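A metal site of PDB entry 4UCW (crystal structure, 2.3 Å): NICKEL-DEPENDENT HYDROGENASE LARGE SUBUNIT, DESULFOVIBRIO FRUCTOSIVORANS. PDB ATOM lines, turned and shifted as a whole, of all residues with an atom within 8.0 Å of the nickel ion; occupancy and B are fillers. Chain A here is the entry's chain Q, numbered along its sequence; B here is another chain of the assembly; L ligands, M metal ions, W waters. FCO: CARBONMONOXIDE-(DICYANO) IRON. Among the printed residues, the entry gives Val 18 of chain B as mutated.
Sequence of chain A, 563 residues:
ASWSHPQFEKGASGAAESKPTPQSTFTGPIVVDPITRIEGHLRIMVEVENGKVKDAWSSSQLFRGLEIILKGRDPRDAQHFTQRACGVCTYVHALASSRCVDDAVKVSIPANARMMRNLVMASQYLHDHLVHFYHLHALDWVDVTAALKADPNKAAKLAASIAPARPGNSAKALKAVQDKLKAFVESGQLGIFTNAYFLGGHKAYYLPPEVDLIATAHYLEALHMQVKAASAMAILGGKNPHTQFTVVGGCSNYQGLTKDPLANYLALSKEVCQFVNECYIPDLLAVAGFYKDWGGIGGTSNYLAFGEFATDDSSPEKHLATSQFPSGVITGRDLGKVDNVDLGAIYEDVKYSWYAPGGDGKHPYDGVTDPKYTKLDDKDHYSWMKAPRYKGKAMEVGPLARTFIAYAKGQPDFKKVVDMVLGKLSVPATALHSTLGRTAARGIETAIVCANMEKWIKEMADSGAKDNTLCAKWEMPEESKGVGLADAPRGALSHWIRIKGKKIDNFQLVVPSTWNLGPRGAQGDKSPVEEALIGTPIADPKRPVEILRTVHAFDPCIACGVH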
ATOM      1  N   GLU A  39      22.844   8.317  18.793  1.00  0.00           N
ATOM      2  CA  GLU A  39      23.513   7.791  17.625  1.00  0.00           C
ATOM      3  C   GLU A  39      25.036   8.111  17.605  1.00  0.00           C
ATOM      4  O   GLU A  39      25.468   9.276  17.734  1.00  0.00           O
ATOM      5  CB  GLU A  39      22.830   8.272  16.371  1.00  0.00           C
ATOM      6  CG  GLU A  39      21.407   7.714  16.208  1.00  0.00           C
ATOM      7  CD  GLU A  39      20.387   8.470  17.069  1.00  0.00           C
ATOM      8  OE1 GLU A  39      20.426   9.731  17.085  1.00  0.00           O
ATOM      9  OE2 GLU A  39      19.598   7.826  17.783  1.00  0.00           O
ATOM     10  N   GLY A  40      25.856   7.078  17.472  1.00  0.00           N
ATOM     11  CA  GLY A  40      27.232   7.333  17.208  1.00  0.00           C
ATOM     12  C   GLY A  40      28.060   7.510  18.456  1.00  0.00           C
ATOM     13  O   GLY A  40      27.575   7.255  19.572  1.00  0.00           O
ATOM     14  N   ARG A  64      34.440   9.031   9.410  1.00  0.00           N
ATOM     15  CA  ARG A  64      34.238   8.149   8.277  1.00  0.00           C
ATOM     16  C   ARG A  64      34.719   8.856   7.002  1.00  0.00           C
ATOM     17  O   ARG A  64      35.516   8.296   6.238  1.00  0.00           O
ATOM     18  CB  ARG A  64      32.783   7.675   8.211  1.00  0.00           C
ATOM     19  CG  ARG A  64      32.454   6.803   9.429  1.00  0.00           C
ATOM     20  CD  ARG A  64      31.031   6.294   9.437  1.00  0.00           C
ATOM     21  NE  ARG A  64      30.153   7.426   9.595  1.00  0.00           N
ATOM     22  CZ  ARG A  64      28.886   7.507   9.196  1.00  0.00           C
ATOM     23  NH1 ARG A  64      28.229   6.475   8.610  1.00  0.00           N
ATOM     24  NH2 ARG A  64      28.268   8.690   9.362  1.00  0.00           N
ATOM     25  N   GLN A  83      23.030   9.357   2.439  1.00  0.00           N
ATOM     26  CA  GLN A  83      21.981   8.813   3.266  1.00  0.00           C
ATOM     27  C   GLN A  83      22.610   7.947   4.363  1.00  0.00           C
ATOM     28  O   GLN A  83      22.151   7.914   5.484  1.00  0.00           O
ATOM     29  CB  GLN A  83      20.924   8.033   2.451  1.00  0.00           C
ATOM     30  CG  GLN A  83      19.839   7.496   3.371  1.00  0.00           C
ATOM     31  CD  GLN A  83      18.523   7.064   2.687  1.00  0.00           C
ATOM     32  OE1 GLN A  83      17.500   7.096   3.326  1.00  0.00           O
ATOM     33  NE2 GLN A  83      18.567   6.638   1.419  1.00  0.00           N
ATOM     34  N   ALA A  85      25.205   8.622   6.010  1.00  0.00           N
ATOM     35  CA  ALA A  85      25.704   9.363   7.126  1.00  0.00           C
ATOM     36  C   ALA A  85      24.979   8.857   8.396  1.00  0.00           C
ATOM     37  O   ALA A  85      25.580   8.842   9.474  1.00  0.00           O
ATOM     38  CB  ALA A  85      25.501  10.868   6.926  1.00  0.00           C
ATOM     39  N   CYS A  86      23.704   8.471   8.268  1.00  0.00           N
ATOM     40  CA  CYS A  86      22.937   8.055   9.398  1.00  0.00           C
ATOM     41  C   CYS A  86      21.679   7.223   9.105  1.00  0.00           C
ATOM     42  O   CYS A  86      20.830   7.578   8.256  1.00  0.00           O
ATOM     43  CB  CYS A  86      22.518   9.285  10.217  1.00  0.00           C
ATOM     44  SG  CYS A  86      21.814   8.876  11.857  1.00  0.00           S
ATOM     45  N   GLY A  87      21.507   6.177   9.917  1.00  0.00           N
ATOM     46  CA  GLY A  87      20.381   5.271   9.807  1.00  0.00           C
ATOM     47  C   GLY A  87      19.190   5.568  10.723  1.00  0.00           C
ATOM     48  O   GLY A  87      18.107   4.952  10.592  1.00  0.00           O
ATOM     49  N   VAL A  88      19.378   6.510  11.640  1.00  0.00           N
ATOM     50  CA  VAL A  88      18.339   6.892  12.548  1.00  0.00           C
ATOM     51  C   VAL A  88      17.555   8.024  11.912  1.00  0.00           C
ATOM     52  O   VAL A  88      16.310   7.838  11.641  1.00  0.00           O
ATOM     53  CB  VAL A  88      18.870   7.233  13.941  1.00  0.00           C
ATOM     54  CG1 VAL A  88      17.750   7.711  14.812  1.00  0.00           C
ATOM     55  CG2 VAL A  88      19.511   6.005  14.545  1.00  0.00           C
ATOM     56  N   CSO A  89      18.239   9.140  11.609  1.00  0.00           N
ATOM     57  CA  CSO A  89      17.665  10.135  10.662  1.00  0.00           C
ATOM     58  CB  CSO A  89      18.149  11.569  10.859  1.00  0.00           C
ATOM     59  SG  CSO A  89      19.904  11.726  10.841  1.00  0.00           S
ATOM     60  C   CSO A  89      17.868   9.622   9.235  1.00  0.00           C
ATOM     61  O   CSO A  89      18.412  10.296   8.384  1.00  0.00           O
ATOM     62  OD  CSO A  89      20.017  12.071  12.575  1.00  0.00           O
ATOM     63  N   THR A  90      17.429   8.378   8.963  1.00  0.00           N
ATOM     64  CA  THR A  90      17.446   7.829   7.619  1.00  0.00           C
ATOM     65  C   THR A  90      16.630   8.777   6.734  1.00  0.00           C
ATOM     66  O   THR A  90      15.836   9.591   7.252  1.00  0.00           O
ATOM     67  CB  THR A  90      16.912   6.372   7.584  1.00  0.00           C
ATOM     68  OG1 THR A  90      17.225   5.765   6.331  1.00  0.00           O
ATOM     69  CG2 THR A  90      15.357   6.294   7.812  1.00  0.00           C
ATOM     70  N   VAL A  92      16.708  11.763   5.517  1.00  0.00           N
ATOM     71  CA  VAL A  92      16.934  13.180   5.475  1.00  0.00           C
ATOM     72  C   VAL A  92      18.200  13.572   4.710  1.00  0.00           C
ATOM     73  O   VAL A  92      18.217  14.621   4.044  1.00  0.00           O
ATOM     74  CB  VAL A  92      16.957  13.843   6.868  1.00  0.00           C
ATOM     75  CG1 VAL A  92      15.694  13.441   7.634  1.00  0.00           C
ATOM     76  CG2 VAL A  92      18.268  13.546   7.626  1.00  0.00           C
ATOM     77  N   HIS A  93      19.260  12.759   4.773  1.00  0.00           N
ATOM     78  CA  HIS A  93      20.414  13.053   3.955  1.00  0.00           C
ATOM     79  C   HIS A  93      20.203  12.794   2.465  1.00  0.00           C
ATOM     80  O   HIS A  93      20.767  13.516   1.600  1.00  0.00           O
ATOM     81  CB  HIS A  93      21.636  12.318   4.458  1.00  0.00           C
ATOM     82  CG  HIS A  93      22.101  12.800   5.789  1.00  0.00           C
ATOM     83  ND1 HIS A  93      22.803  13.976   5.939  1.00  0.00           N
ATOM     84  CD2 HIS A  93      21.972  12.268   7.033  1.00  0.00           C
ATOM     85  CE1 HIS A  93      23.102  14.141   7.224  1.00  0.00           C
ATOM     86  NE2 HIS A  93      22.605  13.127   7.902  1.00  0.00           N
ATOM     87  N   GLN A 124       9.174  10.501   8.952  1.00  0.00           N
ATOM     88  CA  GLN A 124      10.449  10.431   9.661  1.00  0.00           C
ATOM     89  C   GLN A 124      10.389  11.168  11.016  1.00  0.00           C
ATOM     90  O   GLN A 124      10.855  10.640  12.013  1.00  0.00           O
ATOM     91  CB  GLN A 124      11.570  10.931   8.774  1.00  0.00           C
ATOM     92  CG  GLN A 124      12.918  11.001   9.448  1.00  0.00           C
ATOM     93  CD  GLN A 124      13.354   9.631   9.988  1.00  0.00           C
ATOM     94  OE1 GLN A 124      12.957   8.581   9.482  1.00  0.00           O
ATOM     95  NE2 GLN A 124      14.239   9.655  10.987  1.00  0.00           N
ATOM     96  N   ASP A 128      11.130   9.013  14.344  1.00  0.00           N
ATOM     97  CA  ASP A 128      12.365   9.382  15.008  1.00  0.00           C
ATOM     98  C   ASP A 128      12.061   9.955  16.433  1.00  0.00           C
ATOM     99  O   ASP A 128      12.633   9.526  17.406  1.00  0.00           O
ATOM    100  CB  ASP A 128      13.104  10.361  14.074  1.00  0.00           C
ATOM    101  CG  ASP A 128      14.582  10.585  14.439  1.00  0.00           C
ATOM    102  OD1 ASP A 128      15.074  10.376  15.559  1.00  0.00           O
ATOM    103  OD2 ASP A 128      15.291  11.069  13.555  1.00  0.00           O
ATOM    104  N   ALA A 488      15.687  18.694   9.500  1.00  0.00           N
ATOM    105  CA  ALA A 488      15.578  17.312   9.807  1.00  0.00           C
ATOM    106  C   ALA A 488      15.126  17.208  11.267  1.00  0.00           C
ATOM    107  O   ALA A 488      15.043  18.236  11.965  1.00  0.00           O
ATOM    108  CB  ALA A 488      16.930  16.671   9.595  1.00  0.00           C
ATOM    109  N   PRO A 489      14.844  15.973  11.739  1.00  0.00           N
ATOM    110  CA  PRO A 489      14.355  15.850  13.134  1.00  0.00           C
ATOM    111  C   PRO A 489      15.256  16.520  14.155  1.00  0.00           C
ATOM    112  O   PRO A 489      14.773  17.023  15.176  1.00  0.00           O
ATOM    113  CB  PRO A 489      14.305  14.342  13.351  1.00  0.00           C
ATOM    114  CG  PRO A 489      14.018  13.810  11.954  1.00  0.00           C
ATOM    115  CD  PRO A 489      14.863  14.668  11.043  1.00  0.00           C
ATOM    116  N   ARG A 490      16.561  16.549  13.892  1.00  0.00           N
ATOM    117  CA  ARG A 490      17.532  17.169  14.800  1.00  0.00           C
ATOM    118  C   ARG A 490      17.839  18.627  14.459  1.00  0.00           C
ATOM    119  O   ARG A 490      18.541  19.310  15.231  1.00  0.00           O
ATOM    120  CB  ARG A 490      18.810  16.327  14.885  1.00  0.00           C
ATOM    121  CG  ARG A 490      18.713  15.095  15.814  1.00  0.00           C
ATOM    122  CD  ARG A 490      19.524  13.873  15.312  1.00  0.00           C
ATOM    123  NE  ARG A 490      19.068  12.646  15.946  1.00  0.00           N
ATOM    124  CZ  ARG A 490      18.037  11.912  15.513  1.00  0.00           C
ATOM    125  NH1 ARG A 490      17.371  12.255  14.420  1.00  0.00           N
ATOM    126  NH2 ARG A 490      17.659  10.823  16.189  1.00  0.00           N
ATOM    127  N   VAL A 511      25.533  19.542   9.258  1.00  0.00           N
ATOM    128  CA  VAL A 511      24.466  18.708   9.785  1.00  0.00           C
ATOM    129  C   VAL A 511      24.026  19.219  11.181  1.00  0.00           C
ATOM    130  O   VAL A 511      24.796  19.845  11.891  1.00  0.00           O
ATOM    131  CB  VAL A 511      24.905  17.203   9.802  1.00  0.00           C
ATOM    132  CG1 VAL A 511      23.709  16.264  10.047  1.00  0.00           C
ATOM    133  CG2 VAL A 511      25.517  16.801   8.469  1.00  0.00           C
ATOM    134  N   PRO A 512      22.748  19.028  11.545  1.00  0.00           N
ATOM    135  CA  PRO A 512      22.293  19.583  12.778  1.00  0.00           C
ATOM    136  C   PRO A 512      23.172  19.262  13.978  1.00  0.00           C
ATOM    137  O   PRO A 512      23.468  20.155  14.773  1.00  0.00           O
ATOM    138  CB  PRO A 512      20.877  18.954  12.955  1.00  0.00           C
ATOM    139  CG  PRO A 512      20.648  18.142  11.762  1.00  0.00           C
ATOM    140  CD  PRO A 512      21.618  18.627  10.715  1.00  0.00           C
ATOM    141  N   SER A 513      23.531  17.999  14.144  1.00  0.00           N
ATOM    142  CA  SER A 513      24.421  17.639  15.230  1.00  0.00           C
ATOM    143  C   SER A 513      25.781  18.310  15.130  1.00  0.00           C
ATOM    144  O   SER A 513      26.428  18.433  16.154  1.00  0.00           O
ATOM    145  CB  SER A 513      24.562  16.152  15.302  1.00  0.00           C
ATOM    146  OG  SER A 513      23.318  15.652  15.744  1.00  0.00           O
ATOM    147  N   ASP A 555      19.353  15.234  21.361  1.00  0.00           N
ATOM    148  CA  ASP A 555      19.129  14.108  20.426  1.00  0.00           C
ATOM    149  C   ASP A 555      20.378  13.920  19.544  1.00  0.00           C
ATOM    150  O   ASP A 555      20.293  13.976  18.340  1.00  0.00           O
ATOM    151  CB  ASP A 555      17.844  14.388  19.613  1.00  0.00           C
ATOM    152  CG  ASP A 555      17.409  13.222  18.709  1.00  0.00           C
ATOM    153  OD1 ASP A 555      18.008  12.137  18.741  1.00  0.00           O
ATOM    154  OD2 ASP A 555      16.471  13.412  17.909  1.00  0.00           O
ATOM    155  N   PRO A 556      21.550  13.699  20.170  1.00  0.00           N
ATOM    156  CA  PRO A 556      22.769  13.777  19.402  1.00  0.00           C
ATOM    157  C   PRO A 556      22.874  12.602  18.421  1.00  0.00           C
ATOM    158  O   PRO A 556      22.385  11.493  18.739  1.00  0.00           O
ATOM    159  CB  PRO A 556      23.873  13.684  20.485  1.00  0.00           C
ATOM    160  CG  PRO A 556      23.190  14.126  21.720  1.00  0.00           C
ATOM    161  CD  PRO A 556      21.847  13.504  21.594  1.00  0.00           C
ATOM    162  N   CYS A 557      23.463  12.868  17.257  1.00  0.00           N
ATOM    163  CA  CYS A 557      23.877  11.833  16.272  1.00  0.00           C
ATOM    164  C   CYS A 557      25.275  12.182  15.784  1.00  0.00           C
ATOM    165  O   CYS A 557      25.492  13.183  15.114  1.00  0.00           O
ATOM    166  CB  CYS A 557      22.919  11.778  15.098  1.00  0.00           C
ATOM    167  SG  CYS A 557      23.311  10.563  13.867  1.00  0.00           S
ATOM    168  N   ILE A 558      26.239  11.401  16.206  1.00  0.00           N
ATOM    169  CA  ILE A 558      27.643  11.718  15.922  1.00  0.00           C
ATOM    170  C   ILE A 558      27.952  11.304  14.472  1.00  0.00           C
ATOM    171  O   ILE A 558      28.936  11.802  13.844  1.00  0.00           O
ATOM    172  CB  ILE A 558      28.607  11.026  16.940  1.00  0.00           C
ATOM    173  CG1 ILE A 558      28.145  11.225  18.384  1.00  0.00           C
ATOM    174  CG2 ILE A 558      30.056  11.490  16.813  1.00  0.00           C
ATOM    175  CD1 ILE A 558      27.978  12.688  18.821  1.00  0.00           C
ATOM    176  N   ALA A 559      27.154  10.377  13.945  1.00  0.00           N
ATOM    177  CA  ALA A 559      27.445   9.831  12.623  1.00  0.00           C
ATOM    178  C   ALA A 559      27.008  10.913  11.641  1.00  0.00           C
ATOM    179  O   ALA A 559      27.741  11.206  10.675  1.00  0.00           O
ATOM    180  CB  ALA A 559      26.742   8.488  12.404  1.00  0.00           C
ATOM    181  N   CYS A 560      25.841  11.522  11.938  1.00  0.00           N
ATOM    182  CA  CYS A 560      25.362  12.722  11.230  1.00  0.00           C
ATOM    183  C   CYS A 560      26.352  13.841  11.394  1.00  0.00           C
ATOM    184  O   CYS A 560      26.698  14.507  10.410  1.00  0.00           O
ATOM    185  CB  CYS A 560      24.061  13.183  11.805  1.00  0.00           C
ATOM    186  SG  CYS A 560      22.601  12.548  10.980  1.00  0.00           S
ATOM    187  N   GLY A 561      26.820  14.050  12.634  1.00  0.00           N
ATOM    188  CA  GLY A 561      27.678  15.201  12.944  1.00  0.00           C
ATOM    189  C   GLY A 561      29.018  15.240  12.227  1.00  0.00           C
ATOM    190  O   GLY A 561      29.472  16.316  11.789  1.00  0.00           O
ATOM    191  N   CYS B  17      26.250   3.590  11.072  1.00  0.00           N
ATOM    192  CA  CYS B  17      25.323   4.675  10.915  1.00  0.00           C
ATOM    193  C   CYS B  17      24.059   4.352  11.725  1.00  0.00           C
ATOM    194  O   CYS B  17      23.079   5.089  11.678  1.00  0.00           O
ATOM    195  CB  CYS B  17      24.992   4.842   9.426  1.00  0.00           C
ATOM    196  SG  CYS B  17      23.620   3.793   8.833  1.00  0.00           S
ATOM    197  N   VAL B  18      24.068   3.221  12.440  1.00  0.00           N
ATOM    198  CA  VAL B  18      23.015   2.802  13.364  1.00  0.00           C
ATOM    199  C   VAL B  18      21.771   2.278  12.575  1.00  0.00           C
ATOM    200  O   VAL B  18      20.733   1.906  13.156  1.00  0.00           O
ATOM    201  CB  VAL B  18      22.612   3.908  14.397  1.00  0.00           C
ATOM    202  CG1 VAL B  18      21.772   3.328  15.529  1.00  0.00           C
ATOM    203  CG2 VAL B  18      23.834   4.620  15.013  1.00  0.00           C
HETATM  204 FE   FCO L   1      20.674  13.552  11.520  1.00  0.00          FE
HETATM  205  C1  FCO L   1      21.626  14.692  12.710  1.00  0.00           C
HETATM  206  N1  FCO L   1      22.157  15.385  13.445  1.00  0.00           N
HETATM  207  C2  FCO L   1      18.926  14.238  11.870  1.00  0.00           C
HETATM  208  N2  FCO L   1      17.846  14.657  12.097  1.00  0.00           N
HETATM  209  C3  FCO L   1      20.734  14.703  10.215  1.00  0.00           C
HETATM  210  O3  FCO L   1      20.787  15.449   9.364  1.00  0.00           O
HETATM  211 NI    NI M   1      21.584  10.905  12.551  1.00  0.00          NI
HETATM  212  O   HOH W   1      20.747  10.188  14.136  1.00  0.00           O
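Water W1 lies within hydrogen-bond range of OE1 of Glu 39 (3.0 Å) and NE of Arg 490 (3.5 Å).
The nickel ion is bound by water W1 (1.9 Å), OD of CSO 89 (2.0 Å), SG of Cys 86 (2.2 Å), SG of Cys 557 (2.2 Å) and SG of Cys 560 (2.5 Å).
The nickel ion has five donor atoms within binding distance.
The guanidinium group (NH1) of Arg 490 sits close to OD of CSO 89, at 3.2 Å.
The backbone NH (N) of Val 88 lies close to the side-chain sulfur (SG) of Cys 86 (3.4 Å).
N of Cys 557 is in hydrogen-bond range of OG of Ser 513 (3.2 Å).
The side-chain sulfur (SG) of Cys 560 lies close to a ring nitrogen (NE2) of His 93 (3.1 Å).
Of the 29 residues printed, 4 come within 4 Å of the nickel ion.
The nearest printed residue that does not touch the nickel ion is Arg 490 (4.5 Å).
FE of the ligand is bound by OD of CSO 89 (1.9 Å).
FE of the ligand is bound by SG of Cys 560.
The backbone NH of Arg 490 lies within hydrogen-bond range of a nitrogen (N2) of the ligand (2.9 Å).
The guanidinium group (NH1) of Arg 490 sits at hydrogen-bond distance from a nitrogen (N2) of the ligand (3.4 Å).
An oxygen (O3) of the ligand is in hydrogen-bond range of a ring nitrogen (NE2) of His 93 (3.3 Å).
N of Ser 513 sits at hydrogen-bond distance from N1 of the ligand (3.0 Å).
The side-chain hydroxyl (OG) of Ser 513 lies within hydrogen-bond range of a nitrogen (N1) of the ligand (2.6 Å).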
